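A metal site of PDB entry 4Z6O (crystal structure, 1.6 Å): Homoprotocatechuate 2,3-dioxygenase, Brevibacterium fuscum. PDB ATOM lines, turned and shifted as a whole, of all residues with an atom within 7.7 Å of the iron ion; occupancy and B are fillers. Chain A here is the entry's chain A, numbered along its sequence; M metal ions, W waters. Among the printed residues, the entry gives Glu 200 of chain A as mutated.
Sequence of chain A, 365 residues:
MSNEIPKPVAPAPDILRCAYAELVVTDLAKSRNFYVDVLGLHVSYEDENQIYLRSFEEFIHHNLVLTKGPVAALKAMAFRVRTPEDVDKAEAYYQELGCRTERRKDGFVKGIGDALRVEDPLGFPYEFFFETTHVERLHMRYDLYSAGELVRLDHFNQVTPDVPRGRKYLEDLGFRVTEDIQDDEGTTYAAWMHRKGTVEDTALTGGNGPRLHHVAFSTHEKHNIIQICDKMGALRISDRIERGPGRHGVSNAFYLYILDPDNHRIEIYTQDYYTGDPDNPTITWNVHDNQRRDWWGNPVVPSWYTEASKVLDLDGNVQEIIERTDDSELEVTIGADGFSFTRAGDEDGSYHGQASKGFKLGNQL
The iron ion is bound by the side-chain carboxylate (OE1) of Glu 267, water W1, water W3, a ring nitrogen (NE2) of His 214, water W2 and a ring nitrogen (NE2) of His 155. The iron ion has six donor atoms within binding distance.
Water W1 lies within hydrogen-bond range of the side-chain carboxylate of Glu 200 (2.7 Å) and the side-chain carboxylate of Glu 267 (3.3 Å). Water W2 lies within hydrogen-bond range of the side-chain carboxylate (OE1) of Glu 200 (2.5 Å), the side-chain amide nitrogen (ND2) of Asn 157 (2.8 Å) and the indole nitrogen (NE1) of Trp 192 (3.4 Å).
OE2 of Glu 267 lies within hydrogen-bond range of OH of Tyr 257, 3.3 Å away. The side-chain carboxylate (OE2) of Glu 267 is in hydrogen-bond range of a ring nitrogen (NE2) of His 248 (2.8 Å). O of His 214 lies within hydrogen-bond range of N of Asn 157. A ring nitrogen (ND1) of His 214 sits at hydrogen-bond distance from a ring nitrogen (ND1) of His 213. NE2 of His 155 sits close to OE1 of Glu 200 (3.2 Å). A ring nitrogen (ND1) of His 155 is in hydrogen-bond range of the side-chain carboxylate of Asp 154 (2.7 Å). The side-chain carboxylate (OE2) of Glu 200 lies within hydrogen-bond range of the side-chain hydroxyl (OH) of Tyr 269. The indole nitrogen (NE1) of Trp 192 lies close to the side-chain carboxylate (OE1) of Glu 200 (3.5 Å).
OE1 of Glu 200 touches the iron ion, 3.8 Å away. Along chain A the residues within 4 Å of the iron ion span positions 155 to 267. The nearest printed residue that does not touch the iron ion is Tyr 257 (4.1 Å).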
ATOM      1  N   ASP A 154      32.545  32.441  19.467  1.00  0.00           N
ATOM      2  CA  ASP A 154      33.067  31.166  19.080  1.00  0.00           C
ATOM      3  C   ASP A 154      34.053  31.173  17.895  1.00  0.00           C
ATOM      4  O   ASP A 154      35.107  30.489  17.962  1.00  0.00           O
ATOM      5  CB  ASP A 154      31.990  30.127  18.835  1.00  0.00           C
ATOM      6  CG  ASP A 154      32.599  28.718  18.651  1.00  0.00           C
ATOM      7  OD1 ASP A 154      33.123  28.167  19.651  1.00  0.00           O
ATOM      8  OD2 ASP A 154      32.667  28.201  17.506  1.00  0.00           O
ATOM      9  N   HIS A 155      33.666  31.823  16.782  1.00  0.00           N
ATOM     10  CA  HIS A 155      34.467  31.756  15.571  1.00  0.00           C
ATOM     11  C   HIS A 155      34.087  32.795  14.567  1.00  0.00           C
ATOM     12  O   HIS A 155      33.062  33.449  14.678  1.00  0.00           O
ATOM     13  CB  HIS A 155      34.370  30.363  14.913  1.00  0.00           C
ATOM     14  CG  HIS A 155      33.007  30.023  14.384  1.00  0.00           C
ATOM     15  ND1 HIS A 155      32.094  29.305  15.101  1.00  0.00           N
ATOM     16  CD2 HIS A 155      32.445  30.235  13.173  1.00  0.00           C
ATOM     17  CE1 HIS A 155      31.014  29.100  14.384  1.00  0.00           C
ATOM     18  NE2 HIS A 155      31.188  29.676  13.211  1.00  0.00           N
ATOM     19  N   PHE A 156      34.942  32.900  13.543  1.00  0.00           N
ATOM     20  CA  PHE A 156      34.699  33.658  12.340  1.00  0.00           C
ATOM     21  C   PHE A 156      34.583  32.687  11.172  1.00  0.00           C
ATOM     22  O   PHE A 156      35.059  31.531  11.243  1.00  0.00           O
ATOM     23  CB  PHE A 156      35.901  34.544  12.016  1.00  0.00           C
ATOM     24  CG  PHE A 156      36.402  35.375  13.157  1.00  0.00           C
ATOM     25  CD1 PHE A 156      35.561  36.274  13.832  1.00  0.00           C
ATOM     26  CD2 PHE A 156      37.745  35.312  13.528  1.00  0.00           C
ATOM     27  CE1 PHE A 156      36.046  37.062  14.861  1.00  0.00           C
ATOM     28  CE2 PHE A 156      38.241  36.098  14.560  1.00  0.00           C
ATOM     29  CZ  PHE A 156      37.393  36.962  15.233  1.00  0.00           C
ATOM     30  N   ASN A 157      33.977  33.141  10.088  1.00  0.00           N
ATOM     31  CA  ASN A 157      33.976  32.358   8.837  1.00  0.00           C
ATOM     32  C   ASN A 157      34.231  33.295   7.652  1.00  0.00           C
ATOM     33  O   ASN A 157      33.523  34.284   7.447  1.00  0.00           O
ATOM     34  CB  ASN A 157      32.648  31.596   8.697  1.00  0.00           C
ATOM     35  CG  ASN A 157      32.640  30.645   7.529  1.00  0.00           C
ATOM     36  OD1 ASN A 157      32.845  31.037   6.391  1.00  0.00           O
ATOM     37  ND2 ASN A 157      32.399  29.394   7.805  1.00  0.00           N
ATOM     38  N   TRP A 192      37.209  23.902   8.090  1.00  0.00           N
ATOM     39  CA  TRP A 192      37.085  24.446   9.423  1.00  0.00           C
ATOM     40  C   TRP A 192      38.375  24.165  10.142  1.00  0.00           C
ATOM     41  O   TRP A 192      38.929  23.085  10.015  1.00  0.00           O
ATOM     42  CB  TRP A 192      35.944  23.726  10.136  1.00  0.00           C
ATOM     43  CG  TRP A 192      34.585  24.150   9.669  1.00  0.00           C
ATOM     44  CD1 TRP A 192      33.742  25.009  10.315  1.00  0.00           C
ATOM     45  CD2 TRP A 192      33.920  23.797   8.449  1.00  0.00           C
ATOM     46  NE1 TRP A 192      32.595  25.214   9.593  1.00  0.00           N
ATOM     47  CE2 TRP A 192      32.666  24.474   8.434  1.00  0.00           C
ATOM     48  CE3 TRP A 192      34.243  22.950   7.378  1.00  0.00           C
ATOM     49  CZ2 TRP A 192      31.731  24.334   7.394  1.00  0.00           C
ATOM     50  CZ3 TRP A 192      33.322  22.845   6.304  1.00  0.00           C
ATOM     51  CH2 TRP A 192      32.071  23.502   6.353  1.00  0.00           C
ATOM     52  N   GLU A 200      36.146  25.110  15.491  1.00  0.00           N
ATOM     53  CA  GLU A 200      36.642  26.230  14.693  1.00  0.00           C
ATOM     54  C   GLU A 200      36.972  27.452  15.566  1.00  0.00           C
ATOM     55  O   GLU A 200      36.259  27.761  16.533  1.00  0.00           O
ATOM     56  CB  GLU A 200      35.659  26.621  13.613  1.00  0.00           C
ATOM     57  CG  GLU A 200      34.232  26.642  14.121  1.00  0.00           C
ATOM     58  CD  GLU A 200      33.143  26.809  13.051  1.00  0.00           C
ATOM     59  OE1 GLU A 200      33.332  27.572  12.064  1.00  0.00           O
ATOM     60  OE2 GLU A 200      32.066  26.186  13.258  1.00  0.00           O
ATOM     61  N   ALA A 203      37.167  29.657   9.737  1.00  0.00           N
ATOM     62  CA  ALA A 203      36.739  28.674   8.756  1.00  0.00           C
ATOM     63  C   ALA A 203      36.729  29.343   7.407  1.00  0.00           C
ATOM     64  O   ALA A 203      36.610  30.558   7.323  1.00  0.00           O
ATOM     65  CB  ALA A 203      35.357  28.157   9.122  1.00  0.00           C
ATOM     66  N   THR A 205      35.091  29.354   3.547  1.00  0.00           N
ATOM     67  CA  THR A 205      33.973  28.996   2.685  1.00  0.00           C
ATOM     68  C   THR A 205      34.383  29.412   1.294  1.00  0.00           C
ATOM     69  O   THR A 205      34.772  30.548   1.052  1.00  0.00           O
ATOM     70  CB  THR A 205      32.678  29.736   3.105  1.00  0.00           C
ATOM     71  OG1 THR A 205      32.297  29.340   4.431  1.00  0.00           O
ATOM     72  CG2 THR A 205      31.534  29.465   2.104  1.00  0.00           C
ATOM     73  N   HIS A 213      31.989  35.859   5.947  1.00  0.00           N
ATOM     74  CA  HIS A 213      30.728  35.185   5.904  1.00  0.00           C
ATOM     75  C   HIS A 213      29.902  35.465   7.179  1.00  0.00           C
ATOM     76  O   HIS A 213      28.764  35.866   7.064  1.00  0.00           O
ATOM     77  CB  HIS A 213      30.893  33.693   5.686  1.00  0.00           C
ATOM     78  CG  HIS A 213      29.636  33.064   5.233  1.00  0.00           C
ATOM     79  ND1 HIS A 213      28.658  32.694   6.118  1.00  0.00           N
ATOM     80  CD2 HIS A 213      29.138  32.811   4.000  1.00  0.00           C
ATOM     81  CE1 HIS A 213      27.623  32.180   5.455  1.00  0.00           C
ATOM     82  NE2 HIS A 213      27.894  32.247   4.166  1.00  0.00           N
ATOM     83  N   HIS A 214      30.483  35.182   8.334  1.00  0.00           N
ATOM     84  CA  HIS A 214      29.806  35.488   9.565  1.00  0.00           C
ATOM     85  C   HIS A 214      30.758  35.552  10.748  1.00  0.00           C
ATOM     86  O   HIS A 214      31.889  35.106  10.665  1.00  0.00           O
ATOM     87  CB  HIS A 214      28.673  34.460   9.827  1.00  0.00           C
ATOM     88  CG  HIS A 214      29.131  33.038   9.948  1.00  0.00           C
ATOM     89  ND1 HIS A 214      29.085  32.144   8.908  1.00  0.00           N
ATOM     90  CD2 HIS A 214      29.557  32.328  11.020  1.00  0.00           C
ATOM     91  CE1 HIS A 214      29.484  30.955   9.309  1.00  0.00           C
ATOM     92  NE2 HIS A 214      29.776  31.047  10.587  1.00  0.00           N
ATOM     93  N   VAL A 215      30.189  36.029  11.869  1.00  0.00           N
ATOM     94  CA  VAL A 215      30.787  35.973  13.187  1.00  0.00           C
ATOM     95  C   VAL A 215      29.838  35.116  13.998  1.00  0.00           C
ATOM     96  O   VAL A 215      28.620  35.265  13.845  1.00  0.00           O
ATOM     97  CB  VAL A 215      30.919  37.388  13.796  1.00  0.00           C
ATOM     98  CG1 VAL A 215      31.455  37.297  15.183  1.00  0.00           C
ATOM     99  CG2 VAL A 215      31.884  38.211  12.929  1.00  0.00           C
ATOM    100  N   ALA A 216      30.341  34.205  14.831  1.00  0.00           N
ATOM    101  CA  ALA A 216      29.481  33.296  15.573  1.00  0.00           C
ATOM    102  C   ALA A 216      29.625  33.454  17.060  1.00  0.00           C
ATOM    103  O   ALA A 216      30.767  33.497  17.586  1.00  0.00           O
ATOM    104  CB  ALA A 216      29.818  31.855  15.222  1.00  0.00           C
ATOM    105  N   HIS A 248      23.841  21.269  12.522  1.00  0.00           N
ATOM    106  CA  HIS A 248      24.848  21.169  11.486  1.00  0.00           C
ATOM    107  C   HIS A 248      25.269  19.691  11.340  1.00  0.00           C
ATOM    108  O   HIS A 248      25.330  18.924  12.322  1.00  0.00           O
ATOM    109  CB  HIS A 248      26.114  21.948  11.831  1.00  0.00           C
ATOM    110  CG  HIS A 248      26.030  23.428  11.575  1.00  0.00           C
ATOM    111  ND1 HIS A 248      25.651  23.960  10.371  1.00  0.00           N
ATOM    112  CD2 HIS A 248      26.378  24.479  12.361  1.00  0.00           C
ATOM    113  CE1 HIS A 248      25.732  25.283  10.418  1.00  0.00           C
ATOM    114  NE2 HIS A 248      26.180  25.621  11.617  1.00  0.00           N
ATOM    115  N   VAL A 250      28.553  19.178   9.514  1.00  0.00           N
ATOM    116  CA  VAL A 250      29.862  19.700   9.873  1.00  0.00           C
ATOM    117  C   VAL A 250      29.760  20.483  11.215  1.00  0.00           C
ATOM    118  O   VAL A 250      28.980  21.432  11.313  1.00  0.00           O
ATOM    119  CB  VAL A 250      30.417  20.638   8.793  1.00  0.00           C
ATOM    120  CG1 VAL A 250      31.689  21.294   9.295  1.00  0.00           C
ATOM    121  CG2 VAL A 250      30.669  19.941   7.460  1.00  0.00           C
ATOM    122  N   SER A 251      30.523  20.039  12.208  1.00  0.00           N
ATOM    123  CA  SER A 251      30.596  20.618  13.571  1.00  0.00           C
ATOM    124  C   SER A 251      29.642  19.977  14.543  1.00  0.00           C
ATOM    125  O   SER A 251      29.874  20.058  15.754  1.00  0.00           O
ATOM    126  CB  SER A 251      30.410  22.132  13.620  1.00  0.00           C
ATOM    127  OG  SER A 251      29.058  22.534  13.583  1.00  0.00           O
ATOM    128  N   TYR A 255      22.417  25.425  15.480  1.00  0.00           N
ATOM    129  CA  TYR A 255      22.731  26.707  14.845  1.00  0.00           C
ATOM    130  C   TYR A 255      21.553  27.536  14.368  1.00  0.00           C
ATOM    131  O   TYR A 255      20.418  27.040  14.189  1.00  0.00           O
ATOM    132  CB  TYR A 255      23.665  26.464  13.634  1.00  0.00           C
ATOM    133  CG  TYR A 255      22.944  25.918  12.412  1.00  0.00           C
ATOM    134  CD1 TYR A 255      22.316  26.792  11.498  1.00  0.00           C
ATOM    135  CD2 TYR A 255      22.834  24.557  12.177  1.00  0.00           C
ATOM    136  CE1 TYR A 255      21.655  26.309  10.391  1.00  0.00           C
ATOM    137  CE2 TYR A 255      22.153  24.070  11.060  1.00  0.00           C
ATOM    138  CZ  TYR A 255      21.571  24.946  10.176  1.00  0.00           C
ATOM    139  OH  TYR A 255      20.908  24.474   9.089  1.00  0.00           O
ATOM    140  N   TYR A 257      21.272  31.329  11.727  1.00  0.00           N
ATOM    141  CA  TYR A 257      21.895  32.484  11.048  1.00  0.00           C
ATOM    142  C   TYR A 257      20.877  33.618  10.913  1.00  0.00           C
ATOM    143  O   TYR A 257      19.771  33.443  10.346  1.00  0.00           O
ATOM    144  CB  TYR A 257      22.343  32.125   9.626  1.00  0.00           C
ATOM    145  CG  TYR A 257      23.422  31.069   9.595  1.00  0.00           C
ATOM    146  CD1 TYR A 257      24.779  31.379   9.837  1.00  0.00           C
ATOM    147  CD2 TYR A 257      23.102  29.730   9.392  1.00  0.00           C
ATOM    148  CE1 TYR A 257      25.751  30.403   9.838  1.00  0.00           C
ATOM    149  CE2 TYR A 257      24.105  28.754   9.391  1.00  0.00           C
ATOM    150  CZ  TYR A 257      25.407  29.107   9.592  1.00  0.00           C
ATOM    151  OH  TYR A 257      26.367  28.135   9.553  1.00  0.00           O
ATOM    152  N   GLU A 267      26.038  34.089  13.276  1.00  0.00           N
ATOM    153  CA  GLU A 267      25.601  32.753  13.666  1.00  0.00           C
ATOM    154  C   GLU A 267      25.475  32.651  15.170  1.00  0.00           C
ATOM    155  O   GLU A 267      26.309  33.166  15.892  1.00  0.00           O
ATOM    156  CB  GLU A 267      26.599  31.704  13.195  1.00  0.00           C
ATOM    157  CG  GLU A 267      26.103  30.302  13.367  1.00  0.00           C
ATOM    158  CD  GLU A 267      27.059  29.239  12.885  1.00  0.00           C
ATOM    159  OE1 GLU A 267      28.225  29.547  12.616  1.00  0.00           O
ATOM    160  OE2 GLU A 267      26.652  28.068  12.794  1.00  0.00           O
ATOM    161  N   ILE A 268      24.437  31.962  15.625  1.00  0.00           N
ATOM    162  CA  ILE A 268      24.339  31.509  16.984  1.00  0.00           C
ATOM    163  C   ILE A 268      24.481  30.008  17.005  1.00  0.00           C
ATOM    164  O   ILE A 268      23.939  29.315  16.122  1.00  0.00           O
ATOM    165  CB  ILE A 268      22.975  31.902  17.620  1.00  0.00           C
ATOM    166  CG1 ILE A 268      22.480  33.278  17.151  1.00  0.00           C
ATOM    167  CG2 ILE A 268      23.058  31.822  19.137  1.00  0.00           C
ATOM    168  CD1 ILE A 268      23.359  34.386  17.552  1.00  0.00           C
ATOM    169  N   TYR A 269      25.254  29.494  17.940  1.00  0.00           N
ATOM    170  CA  TYR A 269      25.878  28.163  17.802  1.00  0.00           C
ATOM    171  C   TYR A 269      25.966  27.512  19.190  1.00  0.00           C
ATOM    172  O   TYR A 269      26.237  28.199  20.165  1.00  0.00           O
ATOM    173  CB  TYR A 269      27.273  28.420  17.248  1.00  0.00           C
ATOM    174  CG  TYR A 269      28.227  27.334  16.902  1.00  0.00           C
ATOM    175  CD1 TYR A 269      28.286  26.851  15.588  1.00  0.00           C
ATOM    176  CD2 TYR A 269      29.167  26.878  17.834  1.00  0.00           C
ATOM    177  CE1 TYR A 269      29.225  25.941  15.218  1.00  0.00           C
ATOM    178  CE2 TYR A 269      30.146  25.961  17.473  1.00  0.00           C
ATOM    179  CZ  TYR A 269      30.169  25.506  16.154  1.00  0.00           C
ATOM    180  OH  TYR A 269      31.139  24.623  15.763  1.00  0.00           O
ATOM    181  N   ARG A 293      25.425  20.126   5.802  1.00  0.00           N
ATOM    182  CA  ARG A 293      25.300  21.460   6.329  1.00  0.00           C
ATOM    183  C   ARG A 293      24.152  21.541   7.329  1.00  0.00           C
ATOM    184  O   ARG A 293      24.347  21.997   8.408  1.00  0.00           O
ATOM    185  CB  ARG A 293      25.130  22.478   5.205  1.00  0.00           C
ATOM    186  CG  ARG A 293      26.432  22.672   4.398  1.00  0.00           C
ATOM    187  CD  ARG A 293      26.499  24.006   3.701  1.00  0.00           C
ATOM    188  NE  ARG A 293      27.829  24.265   3.114  1.00  0.00           N
ATOM    189  CZ  ARG A 293      28.870  24.813   3.727  1.00  0.00           C
ATOM    190  NH1 ARG A 293      28.816  25.173   5.007  1.00  0.00           N
ATOM    191  NH2 ARG A 293      29.983  25.032   3.049  1.00  0.00           N
ATOM    192  N   TRP A 304      22.667  32.334   1.483  1.00  0.00           N
ATOM    193  CA  TRP A 304      23.695  31.893   2.406  1.00  0.00           C
ATOM    194  C   TRP A 304      25.002  31.669   1.653  1.00  0.00           C
ATOM    195  O   TRP A 304      26.100  31.886   2.195  1.00  0.00           O
ATOM    196  CB  TRP A 304      23.235  30.633   3.157  1.00  0.00           C
ATOM    197  CG  TRP A 304      24.057  30.321   4.376  1.00  0.00           C
ATOM    198  CD1 TRP A 304      23.845  30.781   5.608  1.00  0.00           C
ATOM    199  CD2 TRP A 304      25.269  29.562   4.421  1.00  0.00           C
ATOM    200  NE1 TRP A 304      24.820  30.313   6.468  1.00  0.00           N
ATOM    201  CE2 TRP A 304      25.712  29.578   5.749  1.00  0.00           C
ATOM    202  CE3 TRP A 304      26.009  28.869   3.476  1.00  0.00           C
ATOM    203  CZ2 TRP A 304      26.879  28.937   6.150  1.00  0.00           C
ATOM    204  CZ3 TRP A 304      27.160  28.246   3.871  1.00  0.00           C
ATOM    205  CH2 TRP A 304      27.593  28.298   5.182  1.00  0.00           C
HETATM  206 FE    FE M   1      29.890  29.041  11.500  1.00  0.00          FE
HETATM  207  O   HOH W   1      29.758  27.060  12.181  1.00  0.00           O
HETATM  208  O   HOH W   2      31.675  28.416  10.356  1.00  0.00           O
HETATM  209  O   HOH W   3      28.785  28.051   9.989  1.00  0.00           O
